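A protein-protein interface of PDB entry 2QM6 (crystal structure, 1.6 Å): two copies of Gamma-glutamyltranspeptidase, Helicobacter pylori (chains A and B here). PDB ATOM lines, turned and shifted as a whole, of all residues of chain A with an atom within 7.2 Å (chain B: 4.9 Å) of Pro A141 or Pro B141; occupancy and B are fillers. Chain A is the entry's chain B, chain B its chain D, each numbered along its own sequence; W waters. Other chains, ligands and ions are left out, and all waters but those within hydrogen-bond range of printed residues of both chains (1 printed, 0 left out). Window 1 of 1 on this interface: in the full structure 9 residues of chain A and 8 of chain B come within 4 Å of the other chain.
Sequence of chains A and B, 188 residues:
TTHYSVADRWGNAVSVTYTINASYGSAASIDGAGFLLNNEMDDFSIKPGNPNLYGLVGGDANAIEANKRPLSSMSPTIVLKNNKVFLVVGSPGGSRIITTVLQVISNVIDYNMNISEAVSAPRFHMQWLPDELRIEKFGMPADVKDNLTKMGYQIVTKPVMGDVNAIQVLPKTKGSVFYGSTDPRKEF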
ATOM      1  N   ILE A 135       3.085 -18.418  29.714  1.00  0.00           N
ATOM      2  CA  ILE A 135       2.296 -17.705  28.708  1.00  0.00           C
ATOM      3  C   ILE A 135       1.396 -18.628  27.879  1.00  0.00           C
ATOM      4  O   ILE A 135       1.433 -19.856  28.029  1.00  0.00           O
ATOM      5  CB  ILE A 135       3.191 -16.843  27.773  1.00  0.00           C
ATOM      6  CG1 ILE A 135       4.110 -17.730  26.921  1.00  0.00           C
ATOM      7  CG2 ILE A 135       4.007 -15.822  28.591  1.00  0.00           C
ATOM      8  CD1 ILE A 135       4.744 -16.972  25.729  1.00  0.00           C
ATOM      9  N   PHE A 138       0.154 -17.866  20.977  1.00  0.00           N
ATOM     10  CA  PHE A 138      -0.118 -16.574  20.320  1.00  0.00           C
ATOM     11  C   PHE A 138      -0.231 -15.362  21.247  1.00  0.00           C
ATOM     12  O   PHE A 138      -0.660 -14.289  20.821  1.00  0.00           O
ATOM     13  CB  PHE A 138      -1.358 -16.642  19.409  1.00  0.00           C
ATOM     14  CG  PHE A 138      -1.349 -17.790  18.431  1.00  0.00           C
ATOM     15  CD1 PHE A 138      -0.314 -17.947  17.511  1.00  0.00           C
ATOM     16  CD2 PHE A 138      -2.408 -18.691  18.406  1.00  0.00           C
ATOM     17  CE1 PHE A 138      -0.326 -19.002  16.602  1.00  0.00           C
ATOM     18  CE2 PHE A 138      -2.436 -19.742  17.508  1.00  0.00           C
ATOM     19  CZ  PHE A 138      -1.392 -19.901  16.597  1.00  0.00           C
ATOM     20  N   GLY A 139       0.167 -15.522  22.504  1.00  0.00           N
ATOM     21  CA  GLY A 139      -0.095 -14.507  23.510  1.00  0.00           C
ATOM     22  C   GLY A 139       0.961 -13.436  23.662  1.00  0.00           C
ATOM     23  O   GLY A 139       0.702 -12.370  24.224  1.00  0.00           O
ATOM     24  N   MET A 140       2.164 -13.719  23.170  1.00  0.00           N
ATOM     25  CA  MET A 140       3.284 -12.817  23.356  1.00  0.00           C
ATOM     26  C   MET A 140       4.183 -12.863  22.114  1.00  0.00           C
ATOM     27  O   MET A 140       4.705 -13.920  21.777  1.00  0.00           O
ATOM     28  CB  MET A 140       4.058 -13.245  24.599  1.00  0.00           C
ATOM     29  CG  MET A 140       5.211 -12.358  24.936  1.00  0.00           C
ATOM     30  SD  MET A 140       5.924 -12.874  26.498  1.00  0.00           S
ATOM     31  CE  MET A 140       4.659 -12.259  27.551  1.00  0.00           C
ATOM     32  N   PRO A 141       4.357 -11.719  21.425  1.00  0.00           N
ATOM     33  CA  PRO A 141       5.195 -11.728  20.225  1.00  0.00           C
ATOM     34  C   PRO A 141       6.676 -11.779  20.564  1.00  0.00           C
ATOM     35  O   PRO A 141       7.069 -11.438  21.690  1.00  0.00           O
ATOM     36  CB  PRO A 141       4.859 -10.387  19.559  1.00  0.00           C
ATOM     37  CG  PRO A 141       4.503  -9.511  20.690  1.00  0.00           C
ATOM     38  CD  PRO A 141       3.783 -10.380  21.682  1.00  0.00           C
ATOM     39  N   ALA A 142       7.475 -12.174  19.572  1.00  0.00           N
ATOM     40  CA  ALA A 142       8.920 -12.337  19.705  1.00  0.00           C
ATOM     41  C   ALA A 142       9.608 -11.177  20.427  1.00  0.00           C
ATOM     42  O   ALA A 142      10.436 -11.410  21.315  1.00  0.00           O
ATOM     43  CB  ALA A 142       9.545 -12.544  18.330  1.00  0.00           C
ATOM     44  N   ASP A 143       9.260  -9.937  20.057  1.00  0.00           N
ATOM     45  CA  ASP A 143       9.922  -8.753  20.637  1.00  0.00           C
ATOM     46  C   ASP A 143       9.737  -8.656  22.139  1.00  0.00           C
ATOM     47  O   ASP A 143      10.669  -8.275  22.863  1.00  0.00           O
ATOM     48  CB  ASP A 143       9.392  -7.454  20.014  1.00  0.00           C
ATOM     49  CG  ASP A 143       9.542  -7.413  18.513  1.00  0.00           C
ATOM     50  OD1 ASP A 143       9.069  -8.350  17.839  1.00  0.00           O
ATOM     51  OD2 ASP A 143      10.118  -6.424  18.006  1.00  0.00           O
ATOM     52  N   VAL A 144       8.537  -8.994  22.613  1.00  0.00           N
ATOM     53  CA  VAL A 144       8.242  -8.950  24.050  1.00  0.00           C
ATOM     54  C   VAL A 144       8.939 -10.107  24.773  1.00  0.00           C
ATOM     55  O   VAL A 144       9.562  -9.914  25.825  1.00  0.00           O
ATOM     56  CB  VAL A 144       6.707  -8.960  24.327  1.00  0.00           C
ATOM     57  CG1 VAL A 144       6.422  -9.099  25.806  1.00  0.00           C
ATOM     58  CG2 VAL A 144       6.051  -7.690  23.796  1.00  0.00           C
ATOM     59  N   LYS A 145       8.834 -11.305  24.198  1.00  0.00           N
ATOM     60  CA  LYS A 145       9.538 -12.485  24.745  1.00  0.00           C
ATOM     61  C   LYS A 145      11.042 -12.230  24.869  1.00  0.00           C
ATOM     62  O   LYS A 145      11.642 -12.529  25.912  1.00  0.00           O
ATOM     63  CB  LYS A 145       9.265 -13.731  23.884  1.00  0.00           C
ATOM     64  CG  LYS A 145       7.820 -14.194  23.933  1.00  0.00           C
ATOM     65  CD  LYS A 145       7.596 -15.573  23.336  1.00  0.00           C
ATOM     66  CE  LYS A 145       7.721 -15.586  21.839  1.00  0.00           C
ATOM     67  NZ  LYS A 145       7.072 -16.829  21.286  1.00  0.00           N
ATOM     68  N   ASP A 146      11.647 -11.668  23.822  1.00  0.00           N
ATOM     69  CA  ASP A 146      13.080 -11.384  23.826  1.00  0.00           C
ATOM     70  C   ASP A 146      13.454 -10.433  24.959  1.00  0.00           C
ATOM     71  O   ASP A 146      14.458 -10.637  25.656  1.00  0.00           O
ATOM     72  CB  ASP A 146      13.518 -10.810  22.478  1.00  0.00           C
ATOM     73  CG  ASP A 146      13.587 -11.865  21.378  1.00  0.00           C
ATOM     74  OD1 ASP A 146      13.366 -13.066  21.667  1.00  0.00           O
ATOM     75  OD2 ASP A 146      13.869 -11.475  20.220  1.00  0.00           O
ATOM     76  N   ASN A 147      12.652  -9.388  25.144  1.00  0.00           N
ATOM     77  CA  ASN A 147      12.951  -8.422  26.197  1.00  0.00           C
ATOM     78  C   ASN A 147      12.794  -9.009  27.604  1.00  0.00           C
ATOM     79  O   ASN A 147      13.617  -8.763  28.495  1.00  0.00           O
ATOM     80  CB  ASN A 147      12.153  -7.130  26.004  1.00  0.00           C
ATOM     81  CG  ASN A 147      12.677  -6.302  24.824  1.00  0.00           C
ATOM     82  OD1 ASN A 147      13.814  -6.492  24.382  1.00  0.00           O
ATOM     83  ND2 ASN A 147      11.866  -5.379  24.330  1.00  0.00           N
ATOM     84  N   GLY B 139      -3.574  -3.709  19.389  1.00  0.00           N
ATOM     85  CA  GLY B 139      -3.064  -4.625  18.374  1.00  0.00           C
ATOM     86  C   GLY B 139      -1.574  -4.899  18.386  1.00  0.00           C
ATOM     87  O   GLY B 139      -1.129  -5.926  17.879  1.00  0.00           O
ATOM     88  N   MET B 140      -0.809  -3.988  18.976  1.00  0.00           N
ATOM     89  CA  MET B 140       0.641  -4.056  18.954  1.00  0.00           C
ATOM     90  C   MET B 140       1.200  -3.543  20.282  1.00  0.00           C
ATOM     91  O   MET B 140       0.919  -2.415  20.677  1.00  0.00           O
ATOM     92  CB  MET B 140       1.158  -3.206  17.790  1.00  0.00           C
ATOM     93  CG  MET B 140       2.651  -3.163  17.645  1.00  0.00           C
ATOM     94  SD  MET B 140       3.050  -2.267  16.138  1.00  0.00           S
ATOM     95  CE  MET B 140       2.422  -3.409  14.973  1.00  0.00           C
ATOM     96  N   PRO B 141       1.990  -4.379  20.983  1.00  0.00           N
ATOM     97  CA  PRO B 141       2.542  -3.941  22.269  1.00  0.00           C
ATOM     98  C   PRO B 141       3.720  -2.979  22.122  1.00  0.00           C
ATOM     99  O   PRO B 141       4.350  -2.923  21.055  1.00  0.00           O
ATOM    100  CB  PRO B 141       2.995  -5.252  22.913  1.00  0.00           C
ATOM    101  CG  PRO B 141       3.362  -6.100  21.763  1.00  0.00           C
ATOM    102  CD  PRO B 141       2.351  -5.781  20.685  1.00  0.00           C
ATOM    103  N   ALA B 142       4.001  -2.246  23.203  1.00  0.00           N
ATOM    104  CA  ALA B 142       5.069  -1.239  23.235  1.00  0.00           C
ATOM    105  C   ALA B 142       6.371  -1.734  22.600  1.00  0.00           C
ATOM    106  O   ALA B 142       6.961  -1.043  21.775  1.00  0.00           O
ATOM    107  CB  ALA B 142       5.311  -0.772  24.668  1.00  0.00           C
ATOM    108  N   ASP B 143       6.799  -2.943  22.961  1.00  0.00           N
ATOM    109  CA  ASP B 143       8.103  -3.458  22.524  1.00  0.00           C
ATOM    110  C   ASP B 143       8.166  -3.557  21.000  1.00  0.00           C
ATOM    111  O   ASP B 143       9.175  -3.215  20.379  1.00  0.00           O
ATOM    112  CB  ASP B 143       8.372  -4.834  23.140  1.00  0.00           C
ATOM    113  CG  ASP B 143       8.329  -4.821  24.648  1.00  0.00           C
ATOM    114  OD1 ASP B 143       7.271  -4.465  25.226  1.00  0.00           O
ATOM    115  OD2 ASP B 143       9.360  -5.175  25.259  1.00  0.00           O
ATOM    116  N   VAL B 144       7.078  -4.037  20.399  1.00  0.00           N
ATOM    117  CA  VAL B 144       6.988  -4.170  18.945  1.00  0.00           C
ATOM    118  C   VAL B 144       6.928  -2.796  18.290  1.00  0.00           C
ATOM    119  O   VAL B 144       7.663  -2.542  17.326  1.00  0.00           O
ATOM    120  CB  VAL B 144       5.792  -5.060  18.528  1.00  0.00           C
ATOM    121  CG1 VAL B 144       5.662  -5.120  17.024  1.00  0.00           C
ATOM    122  CG2 VAL B 144       5.955  -6.475  19.084  1.00  0.00           C
ATOM    123  N   LYS B 145       6.095  -1.907  18.828  1.00  0.00           N
ATOM    124  CA  LYS B 145       6.017  -0.536  18.318  1.00  0.00           C
ATOM    125  C   LYS B 145       7.372   0.155  18.367  1.00  0.00           C
ATOM    126  O   LYS B 145       7.756   0.804  17.388  1.00  0.00           O
ATOM    127  CB  LYS B 145       4.975   0.297  19.071  1.00  0.00           C
ATOM    128  CG  LYS B 145       3.551  -0.189  18.889  1.00  0.00           C
ATOM    129  CD  LYS B 145       2.534   0.817  19.401  1.00  0.00           C
ATOM    130  CE  LYS B 145       2.302   0.666  20.881  1.00  0.00           C
ATOM    131  NZ  LYS B 145       1.121   1.469  21.329  1.00  0.00           N
HETATM  132  O   HOH W   1      11.596  -3.164  22.036  1.00  0.00           O
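The side-chain amide nitrogen (ND2) of Asn A147 sits at hydrogen-bond distance from the side-chain carboxylate (OD2) of Asp B143 (2.7 Å).
ND2 of Asn A147 sits close to O of Asp A143 (3.5 Å).
Among the printed residues, pairs that only touch across the chains: Asp A143 with Val B144, Val A144 with Pro B141, Pro A141 with Val B144, Val A144 with Asp B143 and Pro A141 with Pro B141.
Pro B141 touches just these residues of chain A: Pro A141 and Val A144.
Printed residues of chain B within 4 Å of Val A144: Pro B141 (3.7 Å) and Asp B143 (3.7 Å).
Of the printed residues of chain B, Asn A147 touches Asp B143.
Printed residues of chain B within 4 Å of Asp A143: Val B144 (3.7 Å).
Of the printed residues of chain A, Val B144 touches Pro A141 and Asp A143.
Ala B142 touches none of the printed residues of chain A.
Met A140 touches none of the printed residues of chain B.
Printed residues of chain B that touch a printed residue of chain A: Pro B141, Asp B143 and Val B144.
Hydrophobic or aromatic side chains of chain B that line the printed part of chain A: Pro B141 and Val B144.
Of the 11 printed residues of chain A, 4 touch a printed residue of chain B.
Hydrophobic or aromatic side chains of chain A that line the printed part of chain B: Pro A141 and Val A144.
Pro A141 touches its own counterpart, Pro B141.
Pro A141 touches Val B144, and with the chains exchanged Val A144 touches Pro B141.
Asp A143 touches Val B144, and with the chains exchanged Val A144 touches Asp B143.
Positions printed for both chains: 139, 140, 141, 142, 143, 144 and 145.
Of the 6 pairs that touch across the chains among the printed residues, 5 have their exchanged pair printed and touching as well.
Water W1 lies within hydrogen-bond range of O of Asp B143 (2.9 Å) and ND2 of Asn A147 (3.2 Å).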
